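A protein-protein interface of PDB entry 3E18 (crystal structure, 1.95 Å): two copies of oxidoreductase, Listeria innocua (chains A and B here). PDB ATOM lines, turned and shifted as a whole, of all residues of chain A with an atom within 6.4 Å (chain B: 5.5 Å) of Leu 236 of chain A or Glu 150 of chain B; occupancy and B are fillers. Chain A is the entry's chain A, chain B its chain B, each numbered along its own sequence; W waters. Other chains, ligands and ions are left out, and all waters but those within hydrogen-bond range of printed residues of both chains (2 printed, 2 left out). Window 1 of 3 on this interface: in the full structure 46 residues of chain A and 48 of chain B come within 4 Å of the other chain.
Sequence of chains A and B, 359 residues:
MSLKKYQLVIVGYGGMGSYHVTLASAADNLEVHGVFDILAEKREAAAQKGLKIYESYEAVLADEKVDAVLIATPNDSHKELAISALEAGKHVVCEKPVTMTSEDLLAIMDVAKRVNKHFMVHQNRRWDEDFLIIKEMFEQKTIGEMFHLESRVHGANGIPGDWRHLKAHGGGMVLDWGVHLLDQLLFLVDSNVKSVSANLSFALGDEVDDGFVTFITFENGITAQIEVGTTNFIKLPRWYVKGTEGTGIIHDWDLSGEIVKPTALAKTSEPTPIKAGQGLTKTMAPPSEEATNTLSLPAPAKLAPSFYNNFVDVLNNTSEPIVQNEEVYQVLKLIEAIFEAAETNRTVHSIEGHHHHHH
The side-chain amide oxygen of Gln 225 of chain A is in hydrogen-bond range of the side-chain amide nitrogen of Gln 225 of chain B, at 3.1 Å. NH1 of Arg 152 of chain B lies close to NH1 of Arg 152 of chain A. The side-chain amide nitrogen (ND2) of Asn 232 of chain A lies within hydrogen-bond range of the side-chain hydroxyl (OH) of Tyr 240 of chain B (2.9 Å). The side-chain hydroxyl (OH) of Tyr 240 of chain B lies within hydrogen-bond range of the backbone carbonyl oxygen (O) of Ile 234 of chain A, 2.6 Å away.
NE2 of Gln 225 of chain A sits at hydrogen-bond distance from OE1 of Glu 227 of chain A, at 2.9 Å. The backbone NH (N) of Ser 151 of chain B is in hydrogen-bond range of the backbone carbonyl oxygen (O) of Gln 225 of chain B (2.8 Å). N of Gln 225 of chain B is in hydrogen-bond range of O of Leu 149 of chain B, at 2.9 Å. The guanidinium group of Arg 152 of chain A is in salt-bridge range of the side-chain carboxylate of Glu 227 of chain A (3.3 Å). O of Arg 238 of chain B is in hydrogen-bond range of N of Arg 152 of chain B (3.0 Å). A ring nitrogen (ND1) of His 154 of chain A sits at hydrogen-bond distance from the backbone NH (N) of Leu 236 of chain A, at 3.2 Å.
Tyr 240 of chain B touches His 154 of chain A. CD1 of Ile 234 of chain A touches CG2 of Ile 249 of chain B (3.8 Å). Leu 236 of chain A touches Glu 150 of chain B. Pro 237 of chain B touches Leu 236 of chain A (CG to CD2, 3.8 Å). Leu 236 of chain A touches Tyr 240 of chain B (CD2 to CD1, 3.7 Å).
Printed residues of chain B within 4 Å of Arg 152 of chain A: Arg 152 (3.2 Å). Printed residues of chain B within 4 Å of Gln 225 of chain A: Gln 225 (3.1 Å). Glu 227 of chain A touches none of the printed residues of chain B. Of the printed residues of chain B, Ile 234 of chain A touches Tyr 240 and Ile 249. Leu 236 of chain A touches three residues of chain B. Glu 150 of chain B touches just one residue of chain A: Leu 236 (3.5 Å). Of the printed residues of chain A, Ile 249 of chain B touches Ile 234 (3.8 Å). The nearest printed residue of chain B that does not touch Ile 234 of chain A is Val 241 of chain B (6.5 Å).
Hydrophobic or aromatic side chains of chain B within 4 Å of the printed part of chain A: Pro 237, Tyr 240 and Ile 249. Of the 13 printed residues of chain A, 6 touch a printed residue of chain B. Printed residues of chain A that touch a printed residue of chain B: Arg 152, His 154, Gln 225, Asn 232, Ile 234 and Leu 236. Hydrophobic or aromatic side chains of chain A within 4 Å of the printed part of chain B: His 154, Ile 234 and Leu 236. Among the printed residues, no Asp or Glu carboxylate lies within 4 Å of a Lys or Arg side-chain nitrogen of the other chain.
Arg 152 of chain B touches its own counterpart, Arg 152 of chain A. Gln 225 of chain B touches its own counterpart, Gln 225 of chain A. Positions printed for both chains: 152, 225, 237, 238 and 239.
Water W1 lies within hydrogen-bond range of OE2 of Glu 227 of chain A and OE2 of Glu 150 of chain B. Water W2 lies within hydrogen-bond range of OE1 of Glu 227 of chain A (2.8 Å), OE2 of Glu 150 of chain B (3.2 Å) and NE2 of His 148 of chain B (3.5 Å).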
ATOM      1  N   ARG A 152      29.667 -15.600 -27.502  1.00  0.00           N
ATOM      2  CA  ARG A 152      28.965 -15.170 -26.299  1.00  0.00           C
ATOM      3  C   ARG A 152      28.883 -16.305 -25.299  1.00  0.00           C
ATOM      4  O   ARG A 152      28.539 -17.414 -25.655  1.00  0.00           O
ATOM      5  CB  ARG A 152      27.513 -14.751 -26.623  1.00  0.00           C
ATOM      6  CG  ARG A 152      27.350 -13.453 -27.411  1.00  0.00           C
ATOM      7  CD  ARG A 152      25.867 -13.149 -27.680  1.00  0.00           C
ATOM      8  NE  ARG A 152      25.686 -11.859 -28.370  1.00  0.00           N
ATOM      9  CZ  ARG A 152      25.652 -11.689 -29.691  1.00  0.00           C
ATOM     10  NH1 ARG A 152      25.488 -10.474 -30.203  1.00  0.00           N
ATOM     11  NH2 ARG A 152      25.795 -12.721 -30.511  1.00  0.00           N
ATOM     12  N   HIS A 154      26.690 -16.720 -22.001  1.00  0.00           N
ATOM     13  CA  HIS A 154      25.656 -16.119 -21.175  1.00  0.00           C
ATOM     14  C   HIS A 154      25.177 -17.119 -20.134  1.00  0.00           C
ATOM     15  O   HIS A 154      25.148 -18.322 -20.386  1.00  0.00           O
ATOM     16  CB  HIS A 154      24.452 -15.737 -22.043  1.00  0.00           C
ATOM     17  CG  HIS A 154      24.636 -14.478 -22.840  1.00  0.00           C
ATOM     18  ND1 HIS A 154      23.644 -13.973 -23.653  1.00  0.00           N
ATOM     19  CD2 HIS A 154      25.671 -13.608 -22.927  1.00  0.00           C
ATOM     20  CE1 HIS A 154      24.069 -12.861 -24.227  1.00  0.00           C
ATOM     21  NE2 HIS A 154      25.294 -12.613 -23.801  1.00  0.00           N
ATOM     22  N   GLN A 225      32.536  -9.456 -31.953  1.00  0.00           N
ATOM     23  CA  GLN A 225      31.945  -8.985 -30.735  1.00  0.00           C
ATOM     24  C   GLN A 225      32.053 -10.150 -29.781  1.00  0.00           C
ATOM     25  O   GLN A 225      31.631 -11.245 -30.133  1.00  0.00           O
ATOM     26  CB  GLN A 225      30.484  -8.609 -30.946  1.00  0.00           C
ATOM     27  CG  GLN A 225      29.792  -8.131 -29.653  1.00  0.00           C
ATOM     28  CD  GLN A 225      28.403  -7.572 -29.894  1.00  0.00           C
ATOM     29  OE1 GLN A 225      28.125  -7.034 -30.957  1.00  0.00           O
ATOM     30  NE2 GLN A 225      27.513  -7.710 -28.903  1.00  0.00           N
ATOM     31  N   GLU A 227      31.351 -11.459 -25.752  1.00  0.00           N
ATOM     32  CA  GLU A 227      30.491 -11.015 -24.688  1.00  0.00           C
ATOM     33  C   GLU A 227      30.467 -12.128 -23.668  1.00  0.00           C
ATOM     34  O   GLU A 227      30.530 -13.295 -24.036  1.00  0.00           O
ATOM     35  CB  GLU A 227      29.119 -10.829 -25.317  1.00  0.00           C
ATOM     36  CG  GLU A 227      28.079 -10.110 -24.557  1.00  0.00           C
ATOM     37  CD  GLU A 227      26.884  -9.858 -25.450  1.00  0.00           C
ATOM     38  OE1 GLU A 227      26.950  -8.969 -26.334  1.00  0.00           O
ATOM     39  OE2 GLU A 227      25.887 -10.578 -25.285  1.00  0.00           O
ATOM     40  N   ASN A 232      22.008 -13.138 -17.296  1.00  0.00           N
ATOM     41  CA  ASN A 232      21.174 -13.344 -18.466  1.00  0.00           C
ATOM     42  C   ASN A 232      20.300 -14.566 -18.271  1.00  0.00           C
ATOM     43  O   ASN A 232      20.755 -15.695 -18.443  1.00  0.00           O
ATOM     44  CB  ASN A 232      22.047 -13.556 -19.690  1.00  0.00           C
ATOM     45  CG  ASN A 232      23.019 -12.430 -19.901  1.00  0.00           C
ATOM     46  OD1 ASN A 232      23.786 -12.076 -19.005  1.00  0.00           O
ATOM     47  ND2 ASN A 232      22.999 -11.860 -21.095  1.00  0.00           N
ATOM     48  N   ILE A 234      17.921 -15.418 -20.084  1.00  0.00           N
ATOM     49  CA  ILE A 234      17.746 -15.981 -21.401  1.00  0.00           C
ATOM     50  C   ILE A 234      19.089 -15.803 -22.103  1.00  0.00           C
ATOM     51  O   ILE A 234      19.682 -14.731 -22.019  1.00  0.00           O
ATOM     52  CB  ILE A 234      16.601 -15.252 -22.173  1.00  0.00           C
ATOM     53  CG1 ILE A 234      15.255 -15.494 -21.475  1.00  0.00           C
ATOM     54  CG2 ILE A 234      16.542 -15.703 -23.635  1.00  0.00           C
ATOM     55  CD1 ILE A 234      14.096 -14.622 -21.995  1.00  0.00           C
ATOM     56  N   LYS A 235      19.577 -16.870 -22.737  1.00  0.00           N
ATOM     57  CA  LYS A 235      20.886 -16.860 -23.373  1.00  0.00           C
ATOM     58  C   LYS A 235      20.755 -16.582 -24.865  1.00  0.00           C
ATOM     59  O   LYS A 235      19.853 -17.094 -25.519  1.00  0.00           O
ATOM     60  CB  LYS A 235      21.595 -18.201 -23.153  1.00  0.00           C
ATOM     61  CG  LYS A 235      21.757 -18.623 -21.691  1.00  0.00           C
ATOM     62  CD  LYS A 235      22.426 -19.996 -21.585  1.00  0.00           C
ATOM     63  CE  LYS A 235      22.598 -20.449 -20.139  1.00  0.00           C
ATOM     64  NZ  LYS A 235      21.335 -20.951 -19.515  1.00  0.00           N
ATOM     65  N   LEU A 236      21.656 -15.759 -25.396  1.00  0.00           N
ATOM     66  CA  LEU A 236      21.803 -15.600 -26.832  1.00  0.00           C
ATOM     67  C   LEU A 236      22.723 -16.734 -27.319  1.00  0.00           C
ATOM     68  O   LEU A 236      23.334 -17.392 -26.486  1.00  0.00           O
ATOM     69  CB  LEU A 236      22.394 -14.216 -27.168  1.00  0.00           C
ATOM     70  CG  LEU A 236      21.471 -13.000 -26.974  1.00  0.00           C
ATOM     71  CD1 LEU A 236      22.179 -11.715 -27.400  1.00  0.00           C
ATOM     72  CD2 LEU A 236      20.168 -13.151 -27.753  1.00  0.00           C
ATOM     73  N   PRO A 237      22.807 -16.999 -28.650  1.00  0.00           N
ATOM     74  CA  PRO A 237      23.672 -18.113 -29.093  1.00  0.00           C
ATOM     75  C   PRO A 237      25.143 -18.027 -28.690  1.00  0.00           C
ATOM     76  O   PRO A 237      25.707 -16.923 -28.579  1.00  0.00           O
ATOM     77  CB  PRO A 237      23.576 -18.058 -30.635  1.00  0.00           C
ATOM     78  CG  PRO A 237      22.966 -16.770 -30.950  1.00  0.00           C
ATOM     79  CD  PRO A 237      22.091 -16.408 -29.796  1.00  0.00           C
ATOM     80  N   ARG A 238      25.754 -19.199 -28.518  1.00  0.00           N
ATOM     81  CA  ARG A 238      27.182 -19.311 -28.252  1.00  0.00           C
ATOM     82  C   ARG A 238      27.987 -18.686 -29.400  1.00  0.00           C
ATOM     83  O   ARG A 238      28.913 -17.922 -29.147  1.00  0.00           O
ATOM     84  CB  ARG A 238      27.554 -20.782 -28.011  1.00  0.00           C
ATOM     85  CG  ARG A 238      29.034 -21.077 -27.813  1.00  0.00           C
ATOM     86  CD  ARG A 238      29.624 -20.528 -26.524  1.00  0.00           C
ATOM     87  NE  ARG A 238      31.075 -20.669 -26.542  1.00  0.00           N
ATOM     88  CZ  ARG A 238      31.926 -19.799 -27.083  1.00  0.00           C
ATOM     89  NH1 ARG A 238      31.507 -18.664 -27.630  1.00  0.00           N
ATOM     90  NH2 ARG A 238      33.216 -20.060 -27.043  1.00  0.00           N
ATOM     91  N   TRP A 239      27.615 -18.987 -30.643  1.00  0.00           N
ATOM     92  CA  TRP A 239      28.338 -18.452 -31.829  1.00  0.00           C
ATOM     93  C   TRP A 239      27.345 -17.915 -32.850  1.00  0.00           C
ATOM     94  O   TRP A 239      26.289 -18.504 -33.059  1.00  0.00           O
ATOM     95  CB  TRP A 239      29.165 -19.557 -32.477  1.00  0.00           C
ATOM     96  CG  TRP A 239      30.404 -19.962 -31.684  1.00  0.00           C
ATOM     97  CD1 TRP A 239      30.536 -21.036 -30.848  1.00  0.00           C
ATOM     98  CD2 TRP A 239      31.661 -19.296 -31.685  1.00  0.00           C
ATOM     99  NE1 TRP A 239      31.809 -21.079 -30.316  1.00  0.00           N
ATOM    100  CE2 TRP A 239      32.521 -20.022 -30.824  1.00  0.00           C
ATOM    101  CE3 TRP A 239      32.157 -18.159 -32.345  1.00  0.00           C
ATOM    102  CZ2 TRP A 239      33.846 -19.641 -30.595  1.00  0.00           C
ATOM    103  CZ3 TRP A 239      33.465 -17.774 -32.113  1.00  0.00           C
ATOM    104  CH2 TRP A 239      34.299 -18.508 -31.246  1.00  0.00           C
ATOM    105  N   ILE A 250      25.745 -21.441 -33.702  1.00  0.00           N
ATOM    106  CA  ILE A 250      25.831 -22.542 -32.754  1.00  0.00           C
ATOM    107  C   ILE A 250      25.098 -22.055 -31.509  1.00  0.00           C
ATOM    108  O   ILE A 250      25.511 -21.103 -30.861  1.00  0.00           O
ATOM    109  CB  ILE A 250      27.291 -22.972 -32.433  1.00  0.00           C
ATOM    110  CG1 ILE A 250      28.073 -23.272 -33.709  1.00  0.00           C
ATOM    111  CG2 ILE A 250      27.297 -24.205 -31.549  1.00  0.00           C
ATOM    112  CD1 ILE A 250      29.487 -23.764 -33.480  1.00  0.00           C
ATOM    113  N   HIS A 251      23.976 -22.678 -31.197  1.00  0.00           N
ATOM    114  CA  HIS A 251      23.132 -22.187 -30.111  1.00  0.00           C
ATOM    115  C   HIS A 251      23.764 -22.304 -28.739  1.00  0.00           C
ATOM    116  O   HIS A 251      23.760 -21.348 -27.954  1.00  0.00           O
ATOM    117  CB  HIS A 251      21.794 -22.919 -30.118  1.00  0.00           C
ATOM    118  CG  HIS A 251      20.972 -22.641 -31.330  1.00  0.00           C
ATOM    119  ND1 HIS A 251      20.297 -21.454 -31.515  1.00  0.00           N
ATOM    120  CD2 HIS A 251      20.714 -23.398 -32.422  1.00  0.00           C
ATOM    121  CE1 HIS A 251      19.659 -21.491 -32.672  1.00  0.00           C
ATOM    122  NE2 HIS A 251      19.899 -22.658 -33.244  1.00  0.00           N
ATOM    123  N   HIS B 148      19.385  -2.622 -20.124  1.00  0.00           N
ATOM    124  CA  HIS B 148      20.056  -2.945 -21.396  1.00  0.00           C
ATOM    125  C   HIS B 148      19.032  -3.422 -22.420  1.00  0.00           C
ATOM    126  O   HIS B 148      18.230  -4.314 -22.149  1.00  0.00           O
ATOM    127  CB  HIS B 148      21.148  -4.008 -21.195  1.00  0.00           C
ATOM    128  CG  HIS B 148      21.928  -4.316 -22.433  1.00  0.00           C
ATOM    129  ND1 HIS B 148      22.744  -3.389 -23.048  1.00  0.00           N
ATOM    130  CD2 HIS B 148      22.021  -5.445 -23.172  1.00  0.00           C
ATOM    131  CE1 HIS B 148      23.302  -3.933 -24.114  1.00  0.00           C
ATOM    132  NE2 HIS B 148      22.889  -5.182 -24.205  1.00  0.00           N
ATOM    133  N   LEU B 149      19.061  -2.821 -23.600  1.00  0.00           N
ATOM    134  CA  LEU B 149      18.133  -3.176 -24.662  1.00  0.00           C
ATOM    135  C   LEU B 149      18.907  -3.514 -25.928  1.00  0.00           C
ATOM    136  O   LEU B 149      19.840  -2.797 -26.281  1.00  0.00           O
ATOM    137  CB  LEU B 149      17.202  -1.997 -24.960  1.00  0.00           C
ATOM    138  CG  LEU B 149      16.193  -1.543 -23.907  1.00  0.00           C
ATOM    139  CD1 LEU B 149      16.774  -0.427 -23.056  1.00  0.00           C
ATOM    140  CD2 LEU B 149      14.937  -1.071 -24.606  1.00  0.00           C
ATOM    141  N   GLU B 150      18.562  -4.612 -26.591  1.00  0.00           N
ATOM    142  CA  GLU B 150      19.162  -4.904 -27.902  1.00  0.00           C
ATOM    143  C   GLU B 150      18.069  -4.958 -28.958  1.00  0.00           C
ATOM    144  O   GLU B 150      17.125  -5.735 -28.844  1.00  0.00           O
ATOM    145  CB  GLU B 150      20.008  -6.183 -27.875  1.00  0.00           C
ATOM    146  CG  GLU B 150      21.075  -6.147 -26.779  1.00  0.00           C
ATOM    147  CD  GLU B 150      22.063  -7.298 -26.797  1.00  0.00           C
ATOM    148  OE1 GLU B 150      21.925  -8.205 -27.640  1.00  0.00           O
ATOM    149  OE2 GLU B 150      22.990  -7.280 -25.944  1.00  0.00           O
ATOM    150  N   SER B 151      18.196  -4.107 -29.972  1.00  0.00           N
ATOM    151  CA  SER B 151      17.170  -3.956 -31.016  1.00  0.00           C
ATOM    152  C   SER B 151      17.809  -4.210 -32.370  1.00  0.00           C
ATOM    153  O   SER B 151      18.716  -3.477 -32.766  1.00  0.00           O
ATOM    154  CB  SER B 151      16.584  -2.535 -30.988  1.00  0.00           C
ATOM    155  OG  SER B 151      15.590  -2.366 -31.991  1.00  0.00           O
ATOM    156  N   ARG B 152      17.330  -5.254 -33.053  1.00  0.00           N
ATOM    157  CA  ARG B 152      17.956  -5.816 -34.244  1.00  0.00           C
ATOM    158  C   ARG B 152      16.927  -6.045 -35.333  1.00  0.00           C
ATOM    159  O   ARG B 152      15.908  -6.688 -35.098  1.00  0.00           O
ATOM    160  CB  ARG B 152      18.602  -7.166 -33.924  1.00  0.00           C
ATOM    161  CG  ARG B 152      19.832  -7.082 -33.039  1.00  0.00           C
ATOM    162  CD  ARG B 152      20.454  -8.457 -32.906  1.00  0.00           C
ATOM    163  NE  ARG B 152      21.702  -8.394 -32.160  1.00  0.00           N
ATOM    164  CZ  ARG B 152      21.801  -8.580 -30.857  1.00  0.00           C
ATOM    165  NH1 ARG B 152      22.991  -8.499 -30.276  1.00  0.00           N
ATOM    166  NH2 ARG B 152      20.711  -8.841 -30.132  1.00  0.00           N
ATOM    167  N   ALA B 224      22.332   0.509 -24.874  1.00  0.00           N
ATOM    168  CA  ALA B 224      21.560  -0.116 -25.919  1.00  0.00           C
ATOM    169  C   ALA B 224      22.445  -0.504 -27.089  1.00  0.00           C
ATOM    170  O   ALA B 224      23.425   0.168 -27.373  1.00  0.00           O
ATOM    171  CB  ALA B 224      20.420   0.798 -26.374  1.00  0.00           C
ATOM    172  N   GLN B 225      22.099  -1.614 -27.727  1.00  0.00           N
ATOM    173  CA  GLN B 225      22.736  -2.004 -28.977  1.00  0.00           C
ATOM    174  C   GLN B 225      21.671  -2.019 -30.049  1.00  0.00           C
ATOM    175  O   GLN B 225      20.662  -2.702 -29.920  1.00  0.00           O
ATOM    176  CB  GLN B 225      23.406  -3.378 -28.854  1.00  0.00           C
ATOM    177  CG  GLN B 225      24.016  -3.861 -30.159  1.00  0.00           C
ATOM    178  CD  GLN B 225      25.021  -4.982 -29.981  1.00  0.00           C
ATOM    179  OE1 GLN B 225      25.570  -5.168 -28.903  1.00  0.00           O
ATOM    180  NE2 GLN B 225      25.306  -5.703 -31.065  1.00  0.00           N
ATOM    181  N   ILE B 226      21.893  -1.244 -31.107  1.00  0.00           N
ATOM    182  CA  ILE B 226      20.941  -1.137 -32.185  1.00  0.00           C
ATOM    183  C   ILE B 226      21.664  -1.625 -33.443  1.00  0.00           C
ATOM    184  O   ILE B 226      22.778  -1.180 -33.761  1.00  0.00           O
ATOM    185  CB  ILE B 226      20.455   0.330 -32.395  1.00  0.00           C
ATOM    186  CG1 ILE B 226      19.955   1.001 -31.093  1.00  0.00           C
ATOM    187  CG2 ILE B 226      19.460   0.428 -33.565  1.00  0.00           C
ATOM    188  CD1 ILE B 226      18.843   0.283 -30.331  1.00  0.00           C
ATOM    189  N   PRO B 237      17.498 -12.418 -32.587  1.00  0.00           N
ATOM    190  CA  PRO B 237      16.145 -11.962 -32.234  1.00  0.00           C
ATOM    191  C   PRO B 237      15.896 -10.467 -32.448  1.00  0.00           C
ATOM    192  O   PRO B 237      16.830  -9.672 -32.394  1.00  0.00           O
ATOM    193  CB  PRO B 237      16.028 -12.296 -30.739  1.00  0.00           C
ATOM    194  CG  PRO B 237      17.413 -12.457 -30.262  1.00  0.00           C
ATOM    195  CD  PRO B 237      18.201 -12.979 -31.415  1.00  0.00           C
ATOM    196  N   ARG B 238      14.633 -10.116 -32.710  1.00  0.00           N
ATOM    197  CA  ARG B 238      14.206  -8.728 -32.876  1.00  0.00           C
ATOM    198  C   ARG B 238      14.512  -7.891 -31.636  1.00  0.00           C
ATOM    199  O   ARG B 238      15.054  -6.794 -31.738  1.00  0.00           O
ATOM    200  CB  ARG B 238      12.712  -8.687 -33.235  1.00  0.00           C
ATOM    201  CG  ARG B 238      12.088  -7.293 -33.380  1.00  0.00           C
ATOM    202  CD  ARG B 238      12.535  -6.518 -34.616  1.00  0.00           C
ATOM    203  NE  ARG B 238      12.066  -5.131 -34.499  1.00  0.00           N
ATOM    204  CZ  ARG B 238      12.685  -4.171 -33.814  1.00  0.00           C
ATOM    205  NH1 ARG B 238      13.848  -4.394 -33.193  1.00  0.00           N
ATOM    206  NH2 ARG B 238      12.143  -2.963 -33.769  1.00  0.00           N
ATOM    207  N   TRP B 239      14.205  -8.431 -30.463  1.00  0.00           N
ATOM    208  CA  TRP B 239      14.463  -7.733 -29.219  1.00  0.00           C
ATOM    209  C   TRP B 239      15.093  -8.669 -28.208  1.00  0.00           C
ATOM    210  O   TRP B 239      14.675  -9.829 -28.067  1.00  0.00           O
ATOM    211  CB  TRP B 239      13.167  -7.200 -28.615  1.00  0.00           C
ATOM    212  CG  TRP B 239      12.502  -6.086 -29.338  1.00  0.00           C
ATOM    213  CD1 TRP B 239      11.463  -6.180 -30.218  1.00  0.00           C
ATOM    214  CD2 TRP B 239      12.807  -4.684 -29.225  1.00  0.00           C
ATOM    215  NE1 TRP B 239      11.103  -4.932 -30.662  1.00  0.00           N
ATOM    216  CE2 TRP B 239      11.907  -3.993 -30.068  1.00  0.00           C
ATOM    217  CE3 TRP B 239      13.747  -3.949 -28.485  1.00  0.00           C
ATOM    218  CZ2 TRP B 239      11.918  -2.600 -30.201  1.00  0.00           C
ATOM    219  CZ3 TRP B 239      13.751  -2.557 -28.611  1.00  0.00           C
ATOM    220  CH2 TRP B 239      12.844  -1.903 -29.472  1.00  0.00           C
ATOM    221  N   TYR B 240      16.087  -8.151 -27.499  1.00  0.00           N
ATOM    222  CA  TYR B 240      16.681  -8.854 -26.357  1.00  0.00           C
ATOM    223  C   TYR B 240      16.921  -7.794 -25.303  1.00  0.00           C
ATOM    224  O   TYR B 240      17.629  -6.810 -25.549  1.00  0.00           O
ATOM    225  CB  TYR B 240      17.981  -9.564 -26.754  1.00  0.00           C
ATOM    226  CG  TYR B 240      18.672 -10.310 -25.620  1.00  0.00           C
ATOM    227  CD1 TYR B 240      18.156 -11.509 -25.143  1.00  0.00           C
ATOM    228  CD2 TYR B 240      19.844  -9.828 -25.051  1.00  0.00           C
ATOM    229  CE1 TYR B 240      18.775 -12.197 -24.122  1.00  0.00           C
ATOM    230  CE2 TYR B 240      20.482 -10.505 -24.024  1.00  0.00           C
ATOM    231  CZ  TYR B 240      19.931 -11.696 -23.571  1.00  0.00           C
ATOM    232  OH  TYR B 240      20.531 -12.382 -22.567  1.00  0.00           O
ATOM    233  N   VAL B 241      16.277  -7.961 -24.149  1.00  0.00           N
ATOM    234  CA  VAL B 241      16.236  -6.921 -23.116  1.00  0.00           C
ATOM    235  C   VAL B 241      16.541  -7.456 -21.704  1.00  0.00           C
ATOM    236  O   VAL B 241      15.983  -8.473 -21.278  1.00  0.00           O
ATOM    237  CB  VAL B 241      14.888  -6.098 -23.130  1.00  0.00           C
ATOM    238  CG1 VAL B 241      14.745  -5.259 -24.416  1.00  0.00           C
ATOM    239  CG2 VAL B 241      13.671  -6.985 -22.961  1.00  0.00           C
ATOM    240  N   ILE B 249      12.859 -11.671 -24.415  1.00  0.00           N
ATOM    241  CA  ILE B 249      13.238 -11.897 -25.806  1.00  0.00           C
ATOM    242  C   ILE B 249      11.995 -11.819 -26.687  1.00  0.00           C
ATOM    243  O   ILE B 249      10.927 -12.297 -26.310  1.00  0.00           O
ATOM    244  CB  ILE B 249      14.005 -13.261 -25.971  1.00  0.00           C
ATOM    245  CG1 ILE B 249      14.654 -13.396 -27.352  1.00  0.00           C
ATOM    246  CG2 ILE B 249      13.102 -14.484 -25.658  1.00  0.00           C
ATOM    247  CD1 ILE B 249      15.728 -14.519 -27.438  1.00  0.00           C
HETATM  248  O   HOH W   1      23.629  -9.558 -24.511  1.00  0.00           O
HETATM  249  O   HOH W   2      25.920  -6.810 -24.788  1.00  0.00           O
